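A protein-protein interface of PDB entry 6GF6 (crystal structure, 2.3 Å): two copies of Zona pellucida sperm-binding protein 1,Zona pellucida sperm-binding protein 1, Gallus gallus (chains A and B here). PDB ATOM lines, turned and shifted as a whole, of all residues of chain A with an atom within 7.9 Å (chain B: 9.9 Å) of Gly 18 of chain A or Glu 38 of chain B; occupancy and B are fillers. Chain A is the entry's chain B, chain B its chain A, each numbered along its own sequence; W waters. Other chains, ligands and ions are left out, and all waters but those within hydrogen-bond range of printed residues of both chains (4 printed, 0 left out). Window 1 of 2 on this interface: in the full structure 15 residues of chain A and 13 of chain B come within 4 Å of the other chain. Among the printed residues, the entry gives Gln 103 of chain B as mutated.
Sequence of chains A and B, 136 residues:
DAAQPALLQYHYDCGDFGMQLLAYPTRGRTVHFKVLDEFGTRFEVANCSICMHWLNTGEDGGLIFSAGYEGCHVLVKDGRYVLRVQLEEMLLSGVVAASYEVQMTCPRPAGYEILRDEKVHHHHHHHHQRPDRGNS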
ATOM      1  N   ASP A  13     -21.866  -2.661  -8.792  1.00  0.00           N
ATOM      2  CA  ASP A  13     -20.577  -2.115  -9.187  1.00  0.00           C
ATOM      3  C   ASP A  13     -20.782  -0.803  -9.931  1.00  0.00           C
ATOM      4  O   ASP A  13     -21.700  -0.680 -10.752  1.00  0.00           O
ATOM      5  CB  ASP A  13     -19.818  -3.098 -10.094  1.00  0.00           C
ATOM      6  CG  ASP A  13     -19.537  -4.427  -9.416  1.00  0.00           C
ATOM      7  OD1 ASP A  13     -19.160  -4.416  -8.229  1.00  0.00           O
ATOM      8  OD2 ASP A  13     -19.727  -5.485 -10.057  1.00  0.00           O
ATOM      9  N   CYS A  14     -19.940   0.180  -9.627  1.00  0.00           N
ATOM     10  CA  CYS A  14     -19.906   1.436 -10.363  1.00  0.00           C
ATOM     11  C   CYS A  14     -18.801   1.350 -11.406  1.00  0.00           C
ATOM     12  O   CYS A  14     -17.631   1.216 -11.052  1.00  0.00           O
ATOM     13  CB  CYS A  14     -19.656   2.620  -9.430  1.00  0.00           C
ATOM     14  SG  CYS A  14     -20.958   2.902  -8.221  1.00  0.00           S
ATOM     15  N   GLY A  15     -19.171   1.459 -12.681  1.00  0.00           N
ATOM     16  CA  GLY A  15     -18.210   1.483 -13.761  1.00  0.00           C
ATOM     17  C   GLY A  15     -17.962   2.894 -14.263  1.00  0.00           C
ATOM     18  O   GLY A  15     -18.381   3.886 -13.665  1.00  0.00           O
ATOM     19  N   ASP A  16     -17.275   2.972 -15.404  1.00  0.00           N
ATOM     20  CA  ASP A  16     -16.940   4.268 -15.987  1.00  0.00           C
ATOM     21  C   ASP A  16     -18.113   4.861 -16.762  1.00  0.00           C
ATOM     22  O   ASP A  16     -18.235   6.090 -16.838  1.00  0.00           O
ATOM     23  CB  ASP A  16     -15.703   4.152 -16.887  1.00  0.00           C
ATOM     24  CG  ASP A  16     -14.445   3.723 -16.115  1.00  0.00           C
ATOM     25  OD1 ASP A  16     -14.300   4.097 -14.929  1.00  0.00           O
ATOM     26  OD2 ASP A  16     -13.608   2.992 -16.698  1.00  0.00           O
ATOM     27  N   PHE A  17     -18.948   4.020 -17.382  1.00  0.00           N
ATOM     28  CA  PHE A  17     -20.061   4.496 -18.193  1.00  0.00           C
ATOM     29  C   PHE A  17     -21.426   4.085 -17.664  1.00  0.00           C
ATOM     30  O   PHE A  17     -22.431   4.669 -18.076  1.00  0.00           O
ATOM     31  CB  PHE A  17     -19.891   3.982 -19.629  1.00  0.00           C
ATOM     32  CG  PHE A  17     -18.597   4.425 -20.253  1.00  0.00           C
ATOM     33  CD1 PHE A  17     -18.495   5.651 -20.889  1.00  0.00           C
ATOM     34  CD2 PHE A  17     -17.465   3.628 -20.155  1.00  0.00           C
ATOM     35  CE1 PHE A  17     -17.293   6.061 -21.445  1.00  0.00           C
ATOM     36  CE2 PHE A  17     -16.263   4.033 -20.709  1.00  0.00           C
ATOM     37  CZ  PHE A  17     -16.175   5.248 -21.354  1.00  0.00           C
ATOM     38  N   GLY A  18     -21.487   3.109 -16.774  1.00  0.00           N
ATOM     39  CA  GLY A  18     -22.737   2.682 -16.196  1.00  0.00           C
ATOM     40  C   GLY A  18     -22.493   1.905 -14.925  1.00  0.00           C
ATOM     41  O   GLY A  18     -21.399   1.931 -14.360  1.00  0.00           O
ATOM     42  N   MET A  19     -23.532   1.203 -14.482  1.00  0.00           N
ATOM     43  CA  MET A  19     -23.474   0.409 -13.264  1.00  0.00           C
ATOM     44  C   MET A  19     -24.238  -0.888 -13.476  1.00  0.00           C
ATOM     45  O   MET A  19     -25.066  -1.004 -14.383  1.00  0.00           O
ATOM     46  CB  MET A  19     -24.046   1.179 -12.067  1.00  0.00           C
ATOM     47  CG  MET A  19     -25.301   1.969 -12.398  1.00  0.00           C
ATOM     48  SD  MET A  19     -25.873   3.005 -11.040  1.00  0.00           S
ATOM     49  CE  MET A  19     -26.709   4.302 -11.946  1.00  0.00           C
ATOM     50  N   GLN A  20     -23.949  -1.872 -12.626  1.00  0.00           N
ATOM     51  CA  GLN A  20     -24.610  -3.166 -12.694  1.00  0.00           C
ATOM     52  C   GLN A  20     -24.932  -3.655 -11.290  1.00  0.00           C
ATOM     53  O   GLN A  20     -24.148  -3.456 -10.360  1.00  0.00           O
ATOM     54  CB  GLN A  20     -23.753  -4.207 -13.429  1.00  0.00           C
ATOM     55  CG  GLN A  20     -22.435  -4.532 -12.750  1.00  0.00           C
ATOM     56  CD  GLN A  20     -21.765  -5.756 -13.338  1.00  0.00           C
ATOM     57  OE1 GLN A  20     -22.210  -6.296 -14.352  1.00  0.00           O
ATOM     58  NE2 GLN A  20     -20.691  -6.206 -12.701  1.00  0.00           N
ATOM     59  N   MET A  52     -31.692   2.591 -21.788  1.00  0.00           N
ATOM     60  CA  MET A  52     -30.329   2.107 -21.570  1.00  0.00           C
ATOM     61  C   MET A  52     -30.224   1.293 -20.280  1.00  0.00           C
ATOM     62  O   MET A  52     -29.375   1.547 -19.422  1.00  0.00           O
ATOM     63  CB  MET A  52     -29.330   3.267 -21.579  1.00  0.00           C
ATOM     64  CG  MET A  52     -29.398   4.121 -22.836  1.00  0.00           C
ATOM     65  SD  MET A  52     -29.186   3.165 -24.351  1.00  0.00           S
ATOM     66  CE  MET A  52     -29.551   4.402 -25.596  1.00  0.00           C
ATOM     67  N   TRP A  54     -30.778  -3.046 -18.925  1.00  0.00           N
ATOM     68  CA  TRP A  54     -30.848  -4.401 -19.447  1.00  0.00           C
ATOM     69  C   TRP A  54     -30.878  -5.408 -18.305  1.00  0.00           C
ATOM     70  O   TRP A  54     -30.521  -5.105 -17.163  1.00  0.00           O
ATOM     71  CB  TRP A  54     -29.665  -4.704 -20.378  1.00  0.00           C
ATOM     72  CG  TRP A  54     -29.497  -3.721 -21.496  1.00  0.00           C
ATOM     73  CD1 TRP A  54     -30.027  -3.806 -22.751  1.00  0.00           C
ATOM     74  CD2 TRP A  54     -28.747  -2.500 -21.460  1.00  0.00           C
ATOM     75  NE1 TRP A  54     -29.653  -2.715 -23.498  1.00  0.00           N
ATOM     76  CE2 TRP A  54     -28.868  -1.896 -22.728  1.00  0.00           C
ATOM     77  CE3 TRP A  54     -27.986  -1.857 -20.478  1.00  0.00           C
ATOM     78  CZ2 TRP A  54     -28.255  -0.684 -23.041  1.00  0.00           C
ATOM     79  CZ3 TRP A  54     -27.378  -0.653 -20.790  1.00  0.00           C
ATOM     80  CH2 TRP A  54     -27.516  -0.080 -22.060  1.00  0.00           C
ATOM     81  N   SER A  66     -28.176  -4.118 -15.644  1.00  0.00           N
ATOM     82  CA  SER A  66     -27.219  -3.148 -16.168  1.00  0.00           C
ATOM     83  C   SER A  66     -27.919  -1.830 -16.484  1.00  0.00           C
ATOM     84  O   SER A  66     -29.032  -1.831 -17.023  1.00  0.00           O
ATOM     85  CB  SER A  66     -26.552  -3.684 -17.434  1.00  0.00           C
ATOM     86  OG  SER A  66     -25.972  -4.959 -17.198  1.00  0.00           O
ATOM     87  N   ALA A  67     -27.279  -0.708 -16.133  1.00  0.00           N
ATOM     88  CA  ALA A  67     -27.848   0.618 -16.362  1.00  0.00           C
ATOM     89  C   ALA A  67     -26.767   1.614 -16.767  1.00  0.00           C
ATOM     90  O   ALA A  67     -25.786   1.794 -16.039  1.00  0.00           O
ATOM     91  CB  ALA A  67     -28.568   1.113 -15.106  1.00  0.00           C
ATOM     92  N   GLY A  68     -26.956   2.275 -17.910  1.00  0.00           N
ATOM     93  CA  GLY A  68     -26.097   3.392 -18.273  1.00  0.00           C
ATOM     94  C   GLY A  68     -26.369   4.612 -17.412  1.00  0.00           C
ATOM     95  O   GLY A  68     -27.482   4.827 -16.928  1.00  0.00           O
ATOM     96  N   TYR A  69     -25.320   5.417 -17.193  1.00  0.00           N
ATOM     97  CA  TYR A  69     -25.454   6.601 -16.344  1.00  0.00           C
ATOM     98  C   TYR A  69     -26.420   7.634 -16.922  1.00  0.00           C
ATOM     99  O   TYR A  69     -27.018   8.405 -16.167  1.00  0.00           O
ATOM    100  CB  TYR A  69     -24.082   7.252 -16.098  1.00  0.00           C
ATOM    101  CG  TYR A  69     -23.171   6.494 -15.157  1.00  0.00           C
ATOM    102  CD1 TYR A  69     -23.676   5.841 -14.044  1.00  0.00           C
ATOM    103  CD2 TYR A  69     -21.807   6.438 -15.379  1.00  0.00           C
ATOM    104  CE1 TYR A  69     -22.845   5.143 -13.183  1.00  0.00           C
ATOM    105  CE2 TYR A  69     -20.968   5.742 -14.524  1.00  0.00           C
ATOM    106  CZ  TYR A  69     -21.493   5.096 -13.426  1.00  0.00           C
ATOM    107  OH  TYR A  69     -20.661   4.406 -12.567  1.00  0.00           O
ATOM    108  N   GLU A  70     -26.607   7.660 -18.240  1.00  0.00           N
ATOM    109  CA  GLU A  70     -27.475   8.649 -18.870  1.00  0.00           C
ATOM    110  C   GLU A  70     -28.867   8.100 -19.151  1.00  0.00           C
ATOM    111  O   GLU A  70     -29.618   8.698 -19.927  1.00  0.00           O
ATOM    112  CB  GLU A  70     -26.846   9.136 -20.179  1.00  0.00           C
ATOM    113  CG  GLU A  70     -25.446   9.729 -20.043  1.00  0.00           C
ATOM    114  CD  GLU A  70     -25.443  11.097 -19.406  1.00  0.00           C
ATOM    115  OE1 GLU A  70     -26.515  11.735 -19.356  1.00  0.00           O
ATOM    116  OE2 GLU A  70     -24.363  11.537 -18.956  1.00  0.00           O
ATOM    117  N   TYR A  81     -24.427  10.012  -9.500  1.00  0.00           N
ATOM    118  CA  TYR A  81     -25.546   9.336 -10.147  1.00  0.00           C
ATOM    119  C   TYR A  81     -26.262   8.449  -9.143  1.00  0.00           C
ATOM    120  O   TYR A  81     -25.621   7.724  -8.376  1.00  0.00           O
ATOM    121  CB  TYR A  81     -25.073   8.476 -11.316  1.00  0.00           C
ATOM    122  CG  TYR A  81     -24.400   9.225 -12.434  1.00  0.00           C
ATOM    123  CD1 TYR A  81     -25.126  10.055 -13.272  1.00  0.00           C
ATOM    124  CD2 TYR A  81     -23.035   9.093 -12.663  1.00  0.00           C
ATOM    125  CE1 TYR A  81     -24.512  10.736 -14.303  1.00  0.00           C
ATOM    126  CE2 TYR A  81     -22.420   9.770 -13.688  1.00  0.00           C
ATOM    127  CZ  TYR A  81     -23.165  10.588 -14.503  1.00  0.00           C
ATOM    128  OH  TYR A  81     -22.558  11.267 -15.527  1.00  0.00           O
ATOM    129  N   MET A 104     -28.450   2.685  -5.866  1.00  0.00           N
ATOM    130  CA  MET A 104     -27.126   2.601  -6.458  1.00  0.00           C
ATOM    131  C   MET A 104     -26.577   4.013  -6.600  1.00  0.00           C
ATOM    132  O   MET A 104     -27.125   4.831  -7.349  1.00  0.00           O
ATOM    133  CB  MET A 104     -27.185   1.875  -7.801  1.00  0.00           C
ATOM    134  CG  MET A 104     -27.707   0.442  -7.696  1.00  0.00           C
ATOM    135  SD  MET A 104     -28.230  -0.280  -9.272  1.00  0.00           S
ATOM    136  CE  MET A 104     -26.671  -0.624 -10.063  1.00  0.00           C
ATOM    137  N   CYS A 106     -23.206   6.244  -7.482  1.00  0.00           N
ATOM    138  CA  CYS A 106     -21.942   6.140  -8.187  1.00  0.00           C
ATOM    139  C   CYS A 106     -21.381   7.534  -8.421  1.00  0.00           C
ATOM    140  O   CYS A 106     -22.144   8.492  -8.593  1.00  0.00           O
ATOM    141  CB  CYS A 106     -22.098   5.398  -9.522  1.00  0.00           C
ATOM    142  SG  CYS A 106     -22.509   3.641  -9.312  1.00  0.00           S
ATOM    143  N   VAL B  35     -23.072  -7.918 -27.931  1.00  0.00           N
ATOM    144  CA  VAL B  35     -22.443  -6.695 -27.458  1.00  0.00           C
ATOM    145  C   VAL B  35     -21.874  -6.952 -26.073  1.00  0.00           C
ATOM    146  O   VAL B  35     -22.488  -7.644 -25.249  1.00  0.00           O
ATOM    147  CB  VAL B  35     -23.450  -5.531 -27.457  1.00  0.00           C
ATOM    148  CG1 VAL B  35     -22.870  -4.305 -26.759  1.00  0.00           C
ATOM    149  CG2 VAL B  35     -23.851  -5.189 -28.885  1.00  0.00           C
ATOM    150  N   LEU B  36     -20.692  -6.404 -25.824  1.00  0.00           N
ATOM    151  CA  LEU B  36     -19.989  -6.547 -24.558  1.00  0.00           C
ATOM    152  C   LEU B  36     -19.944  -5.193 -23.872  1.00  0.00           C
ATOM    153  O   LEU B  36     -19.588  -4.194 -24.502  1.00  0.00           O
ATOM    154  CB  LEU B  36     -18.551  -7.038 -24.789  1.00  0.00           C
ATOM    155  CG  LEU B  36     -18.387  -8.274 -25.673  1.00  0.00           C
ATOM    156  CD1 LEU B  36     -16.914  -8.588 -25.897  1.00  0.00           C
ATOM    157  CD2 LEU B  36     -19.085  -9.463 -25.048  1.00  0.00           C
ATOM    158  N   ASP B  37     -20.242  -5.159 -22.577  1.00  0.00           N
ATOM    159  CA  ASP B  37     -20.120  -3.919 -21.824  1.00  0.00           C
ATOM    160  C   ASP B  37     -18.861  -3.967 -20.962  1.00  0.00           C
ATOM    161  O   ASP B  37     -18.126  -4.955 -20.948  1.00  0.00           O
ATOM    162  CB  ASP B  37     -21.380  -3.650 -20.988  1.00  0.00           C
ATOM    163  CG  ASP B  37     -21.517  -4.567 -19.782  1.00  0.00           C
ATOM    164  OD1 ASP B  37     -20.682  -5.464 -19.580  1.00  0.00           O
ATOM    165  OD2 ASP B  37     -22.482  -4.366 -19.009  1.00  0.00           O
ATOM    166  N   GLU B  38     -18.608  -2.879 -20.232  1.00  0.00           N
ATOM    167  CA  GLU B  38     -17.371  -2.762 -19.466  1.00  0.00           C
ATOM    168  C   GLU B  38     -17.272  -3.777 -18.334  1.00  0.00           C
ATOM    169  O   GLU B  38     -16.196  -3.894 -17.736  1.00  0.00           O
ATOM    170  CB  GLU B  38     -17.234  -1.348 -18.884  1.00  0.00           C
ATOM    171  CG  GLU B  38     -18.318  -0.963 -17.880  1.00  0.00           C
ATOM    172  CD  GLU B  38     -18.148   0.448 -17.334  1.00  0.00           C
ATOM    173  OE1 GLU B  38     -19.145   1.219 -17.349  1.00  0.00           O
ATOM    174  OE2 GLU B  38     -17.016   0.787 -16.900  1.00  0.00           O
ATOM    175  N   PHE B  39     -18.356  -4.492 -18.017  1.00  0.00           N
ATOM    176  CA  PHE B  39     -18.352  -5.501 -16.965  1.00  0.00           C
ATOM    177  C   PHE B  39     -18.245  -6.902 -17.523  1.00  0.00           C
ATOM    178  O   PHE B  39     -18.379  -7.872 -16.769  1.00  0.00           O
ATOM    179  CB  PHE B  39     -19.610  -5.397 -16.095  1.00  0.00           C
ATOM    180  CG  PHE B  39     -19.849  -4.021 -15.526  1.00  0.00           C
ATOM    181  CD1 PHE B  39     -19.101  -3.564 -14.456  1.00  0.00           C
ATOM    182  CD2 PHE B  39     -20.852  -3.208 -16.033  1.00  0.00           C
ATOM    183  CE1 PHE B  39     -19.322  -2.315 -13.923  1.00  0.00           C
ATOM    184  CE2 PHE B  39     -21.079  -1.954 -15.502  1.00  0.00           C
ATOM    185  CZ  PHE B  39     -20.316  -1.508 -14.445  1.00  0.00           C
ATOM    186  N   GLY B  40     -18.048  -7.031 -18.830  1.00  0.00           N
ATOM    187  CA  GLY B  40     -17.936  -8.329 -19.450  1.00  0.00           C
ATOM    188  C   GLY B  40     -19.249  -9.017 -19.731  1.00  0.00           C
ATOM    189  O   GLY B  40     -19.240 -10.177 -20.151  1.00  0.00           O
ATOM    190  N   THR B  41     -20.375  -8.349 -19.504  1.00  0.00           N
ATOM    191  CA  THR B  41     -21.669  -8.938 -19.812  1.00  0.00           C
ATOM    192  C   THR B  41     -21.902  -8.970 -21.317  1.00  0.00           C
ATOM    193  O   THR B  41     -21.550  -8.033 -22.038  1.00  0.00           O
ATOM    194  CB  THR B  41     -22.777  -8.156 -19.115  1.00  0.00           C
ATOM    195  OG1 THR B  41     -22.496  -8.106 -17.714  1.00  0.00           O
ATOM    196  CG2 THR B  41     -24.139  -8.821 -19.334  1.00  0.00           C
ATOM    197  N   ARG B  42     -22.535 -10.041 -21.776  1.00  0.00           N
ATOM    198  CA  ARG B  42     -22.783 -10.305 -23.188  1.00  0.00           C
ATOM    199  C   ARG B  42     -24.266 -10.111 -23.495  1.00  0.00           C
ATOM    200  O   ARG B  42     -25.123 -10.708 -22.834  1.00  0.00           O
ATOM    201  CB  ARG B  42     -22.310 -11.717 -23.540  1.00  0.00           C
ATOM    202  CG  ARG B  42     -20.780 -11.864 -23.468  1.00  0.00           C
ATOM    203  CD  ARG B  42     -20.305 -13.252 -23.069  1.00  0.00           C
ATOM    204  NE  ARG B  42     -20.722 -14.295 -24.003  1.00  0.00           N
ATOM    205  CZ  ARG B  42     -21.710 -15.163 -23.788  1.00  0.00           C
ATOM    206  NH1 ARG B  42     -22.423 -15.131 -22.667  1.00  0.00           N
ATOM    207  NH2 ARG B  42     -21.991 -16.070 -24.709  1.00  0.00           N
ATOM    208  N   PHE B  43     -24.567  -9.191 -24.410  1.00  0.00           N
ATOM    209  CA  PHE B  43     -25.934  -8.864 -24.788  1.00  0.00           C
ATOM    210  C   PHE B  43     -26.211  -9.401 -26.186  1.00  0.00           C
ATOM    211  O   PHE B  43     -25.662  -8.885 -27.166  1.00  0.00           O
ATOM    212  CB  PHE B  43     -26.146  -7.350 -24.737  1.00  0.00           C
ATOM    213  CG  PHE B  43     -25.866  -6.766 -23.394  1.00  0.00           C
ATOM    214  CD1 PHE B  43     -24.575  -6.430 -23.039  1.00  0.00           C
ATOM    215  CD2 PHE B  43     -26.876  -6.589 -22.469  1.00  0.00           C
ATOM    216  CE1 PHE B  43     -24.298  -5.908 -21.783  1.00  0.00           C
ATOM    217  CE2 PHE B  43     -26.603  -6.062 -21.215  1.00  0.00           C
ATOM    218  CZ  PHE B  43     -25.317  -5.724 -20.875  1.00  0.00           C
ATOM    219  N   HIS B  73     -25.570   0.858 -26.145  1.00  0.00           N
ATOM    220  CA  HIS B  73     -24.217   0.455 -25.773  1.00  0.00           C
ATOM    221  C   HIS B  73     -23.123   1.078 -26.633  1.00  0.00           C
ATOM    222  O   HIS B  73     -21.949   0.799 -26.392  1.00  0.00           O
ATOM    223  CB  HIS B  73     -24.017  -1.072 -25.774  1.00  0.00           C
ATOM    224  CG  HIS B  73     -24.655  -1.773 -24.615  1.00  0.00           C
ATOM    225  ND1 HIS B  73     -25.662  -2.706 -24.761  1.00  0.00           N
ATOM    226  CD2 HIS B  73     -24.404  -1.699 -23.285  1.00  0.00           C
ATOM    227  CE1 HIS B  73     -26.015  -3.164 -23.572  1.00  0.00           C
ATOM    228  NE2 HIS B  73     -25.268  -2.566 -22.659  1.00  0.00           N
ATOM    229  N   LEU B  75     -20.680   3.900 -27.175  1.00  0.00           N
ATOM    230  CA  LEU B  75     -20.130   4.916 -26.298  1.00  0.00           C
ATOM    231  C   LEU B  75     -19.347   5.936 -27.111  1.00  0.00           C
ATOM    232  O   LEU B  75     -18.851   5.643 -28.203  1.00  0.00           O
ATOM    233  CB  LEU B  75     -19.226   4.283 -25.231  1.00  0.00           C
ATOM    234  CG  LEU B  75     -19.887   3.194 -24.372  1.00  0.00           C
ATOM    235  CD1 LEU B  75     -18.860   2.457 -23.530  1.00  0.00           C
ATOM    236  CD2 LEU B  75     -20.972   3.783 -23.485  1.00  0.00           C
ATOM    237  N   LYS B  77     -15.984   7.944 -26.961  1.00  0.00           N
ATOM    238  CA  LYS B  77     -14.682   7.923 -26.306  1.00  0.00           C
ATOM    239  C   LYS B  77     -13.684   8.616 -27.217  1.00  0.00           C
ATOM    240  O   LYS B  77     -13.544   8.236 -28.383  1.00  0.00           O
ATOM    241  CB  LYS B  77     -14.241   6.483 -26.007  1.00  0.00           C
ATOM    242  CG  LYS B  77     -15.185   5.740 -25.068  1.00  0.00           C
ATOM    243  CD  LYS B  77     -14.815   4.262 -24.895  1.00  0.00           C
ATOM    244  CE  LYS B  77     -13.501   4.068 -24.144  1.00  0.00           C
ATOM    245  NZ  LYS B  77     -13.267   2.634 -23.791  1.00  0.00           N
ATOM    246  N   VAL B  82     -17.730   4.038 -30.142  1.00  0.00           N
ATOM    247  CA  VAL B  82     -17.046   2.779 -29.863  1.00  0.00           C
ATOM    248  C   VAL B  82     -18.063   1.735 -29.434  1.00  0.00           C
ATOM    249  O   VAL B  82     -18.898   1.995 -28.562  1.00  0.00           O
ATOM    250  CB  VAL B  82     -15.956   2.949 -28.788  1.00  0.00           C
ATOM    251  CG1 VAL B  82     -15.242   1.645 -28.555  1.00  0.00           C
ATOM    252  CG2 VAL B  82     -14.963   4.024 -29.214  1.00  0.00           C
ATOM    253  N   LEU B  83     -17.994   0.563 -30.053  1.00  0.00           N
ATOM    254  CA  LEU B  83     -18.851  -0.557 -29.697  1.00  0.00           C
ATOM    255  C   LEU B  83     -18.001  -1.819 -29.711  1.00  0.00           C
ATOM    256  O   LEU B  83     -17.300  -2.080 -30.692  1.00  0.00           O
ATOM    257  CB  LEU B  83     -20.034  -0.675 -30.665  1.00  0.00           C
ATOM    258  CG  LEU B  83     -21.080  -1.752 -30.355  1.00  0.00           C
ATOM    259  CD1 LEU B  83     -21.834  -1.432 -29.060  1.00  0.00           C
ATOM    260  CD2 LEU B  83     -22.056  -1.907 -31.502  1.00  0.00           C
ATOM    261  N   ARG B  84     -18.025  -2.568 -28.611  1.00  0.00           N
ATOM    262  CA  ARG B  84     -17.265  -3.807 -28.489  1.00  0.00           C
ATOM    263  C   ARG B  84     -18.206  -4.981 -28.734  1.00  0.00           C
ATOM    264  O   ARG B  84     -19.242  -5.100 -28.071  1.00  0.00           O
ATOM    265  CB  ARG B  84     -16.614  -3.897 -27.103  1.00  0.00           C
ATOM    266  CG  ARG B  84     -15.397  -4.821 -27.010  1.00  0.00           C
ATOM    267  CD  ARG B  84     -14.532  -4.508 -25.775  1.00  0.00           C
ATOM    268  NE  ARG B  84     -15.222  -4.790 -24.515  1.00  0.00           N
ATOM    269  CZ  ARG B  84     -15.082  -5.906 -23.803  1.00  0.00           C
ATOM    270  NH1 ARG B  84     -15.762  -6.061 -22.673  1.00  0.00           N
ATOM    271  NH2 ARG B  84     -14.262  -6.871 -24.202  1.00  0.00           N
ATOM    272  N   GLU B 101     -13.464 -11.300 -31.048  1.00  0.00           N
ATOM    273  CA  GLU B 101     -13.804 -10.022 -30.442  1.00  0.00           C
ATOM    274  C   GLU B 101     -13.236  -8.893 -31.288  1.00  0.00           C
ATOM    275  O   GLU B 101     -12.084  -8.959 -31.735  1.00  0.00           O
ATOM    276  CB  GLU B 101     -13.273  -9.936 -29.013  1.00  0.00           C
ATOM    277  CG  GLU B 101     -13.574  -8.622 -28.324  1.00  0.00           C
ATOM    278  CD  GLU B 101     -13.153  -8.634 -26.865  1.00  0.00           C
ATOM    279  OE1 GLU B 101     -13.344  -9.680 -26.204  1.00  0.00           O
ATOM    280  OE2 GLU B 101     -12.625  -7.607 -26.382  1.00  0.00           O
ATOM    281  N   GLN B 103     -13.317  -4.432 -31.625  1.00  0.00           N
ATOM    282  CA  GLN B 103     -13.699  -3.117 -31.131  1.00  0.00           C
ATOM    283  C   GLN B 103     -13.912  -2.219 -32.342  1.00  0.00           C
ATOM    284  O   GLN B 103     -12.957  -1.876 -33.049  1.00  0.00           O
ATOM    285  CB  GLN B 103     -12.651  -2.533 -30.187  1.00  0.00           C
ATOM    286  CG  GLN B 103     -13.205  -1.355 -29.397  1.00  0.00           C
ATOM    287  CD  GLN B 103     -12.187  -0.713 -28.484  1.00  0.00           C
ATOM    288  OE1 GLN B 103     -12.445  -0.507 -27.300  1.00  0.00           O
ATOM    289  NE2 GLN B 103     -11.028  -0.373 -29.036  1.00  0.00           N
HETATM  290  O   HOH W   1     -21.380   0.466 -18.741  1.00  0.00           O
HETATM  291  O   HOH W   2     -23.461  -5.833 -16.805  1.00  0.00           O
HETATM  292  O   HOH W   3     -14.676   1.002 -18.691  1.00  0.00           O
HETATM  293  O   HOH W   4     -26.221   2.984 -24.356  1.00  0.00           O
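The side-chain carboxylate (OE1) of Glu 38 of chain B is in hydrogen-bond range of the backbone NH (N) of Phe 17 of chain A, 2.8 Å away.
OE2 of Glu 38 of chain B lies within hydrogen-bond range of N of Asp 16 of chain A, 2.7 Å away.
The side-chain carboxylate (OE1) of Glu 38 of chain B sits at hydrogen-bond distance from the backbone NH (N) of Gly 18 of chain A (3.1 Å).
The backbone carbonyl oxygen (O) of Val 35 of chain B sits at hydrogen-bond distance from the backbone NH (N) of Phe 43 of chain B.
O of Gly 15 of chain A sits at hydrogen-bond distance from OH of Tyr 69 of chain A (2.6 Å).
O of Phe 17 of chain A sits at hydrogen-bond distance from N of Tyr 69 of chain A.
O of Asp 37 of chain B lies within hydrogen-bond range of NH1 of Arg 84 of chain B, 3.1 Å away.
N of Asp 13 of chain A sits at hydrogen-bond distance from O of Gln 20 of chain A.
N of Trp 54 of chain A is in hydrogen-bond range of O of Ser 66 of chain A (2.9 Å).
Among the printed residues, pairs that only touch across the chains: Asp 13 of chain A with Phe 39 of chain B (3.9 Å), Gly 15 of chain A with Glu 38 of chain B (3.4 Å), Gly 15 of chain A with Phe 39 of chain B (3.6 Å), Phe 17 of chain A with Leu 75 of chain B (3.8 Å), Phe 17 of chain A with Lys 77 of chain B (3.9 Å), Gly 18 of chain A with Phe 39 of chain B (3.6 Å), Met 19 of chain A with Phe 39 of chain B (3.9 Å), Gln 20 of chain A with Phe 39 of chain B (3.3 Å), Gln 20 of chain A with Thr 41 of chain B (3.8 Å), Trp 54 of chain A with Phe 43 of chain B (3.5 Å), Trp 54 of chain A with His 73 of chain B (3.2 Å), Ser 66 of chain A with Asp 37 of chain B (3.98 Å) and Ser 66 of chain A with Phe 43 of chain B (3.8 Å).
Of the printed residues of chain B, Asp 13 of chain A touches Phe 39 (3.9 Å).
Of the printed residues of chain B, Gly 15 of chain A touches Glu 38 and Phe 39.
Asp 16 of chain A touches one residue of chain B.
Gly 18 of chain A touches two residues of chain B.
Printed residues of chain B within 4 Å of Ser 66 of chain A: Asp 37 and Phe 43.
Ala 67 of chain A touches none of the printed residues of chain B.
No residue of chain B comes within 4 Å of Gly 68 of chain A.
Met 104 of chain A touches none of the printed residues of chain B.
Of the printed residues of chain A, Glu 38 of chain B touches Gly 15, Asp 16, Phe 17 and Gly 18.
Of the printed residues of chain A, Leu 75 of chain B touches Phe 17.
The nearest residue of chain B that does not touch Gly 18 of chain A is Leu 75 of chain B (6.8 Å).
The nearest residue of chain A that does not touch Glu 38 of chain B is Met 19 of chain A (5.2 Å).
The nearest printed residue of chain A that does not touch Phe 39 of chain B is Cys 14 of chain A (4.4 Å).
Hydrophobic or aromatic side chains of chain B that line the printed part of chain A: Phe 39, Phe 43, His 73 and Leu 75.
Of the 18 printed residues of chain A, 9 touch a printed residue of chain B.
No position is printed for both chains.
Water W2 lies within hydrogen-bond range of the side-chain hydroxyl (OG1) of Thr 41 of chain B (2.6 Å), the side-chain hydroxyl (OG) of Ser 66 of chain A (2.7 Å), the side-chain amide oxygen (OE1) of Gln 20 of chain A (2.8 Å) and the side-chain carboxylate (OD2) of Asp 37 of chain B (2.8 Å).
Water W1 lies within hydrogen-bond range of OE1 of Glu 38 of chain B (2.7 Å) and N of Gly 18 of chain A (3.3 Å).
Water W4 bridges the backbone NH of His 73 of chain B (2.9 Å) and the side-chain sulfur of Met 52 of chain A (3.0 Å).
Water W3 lies within hydrogen-bond range of the side-chain carboxylate of Glu 38 of chain B (3.0 Å) and the side-chain carboxylate of Asp 16 of chain A (3.0 Å).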
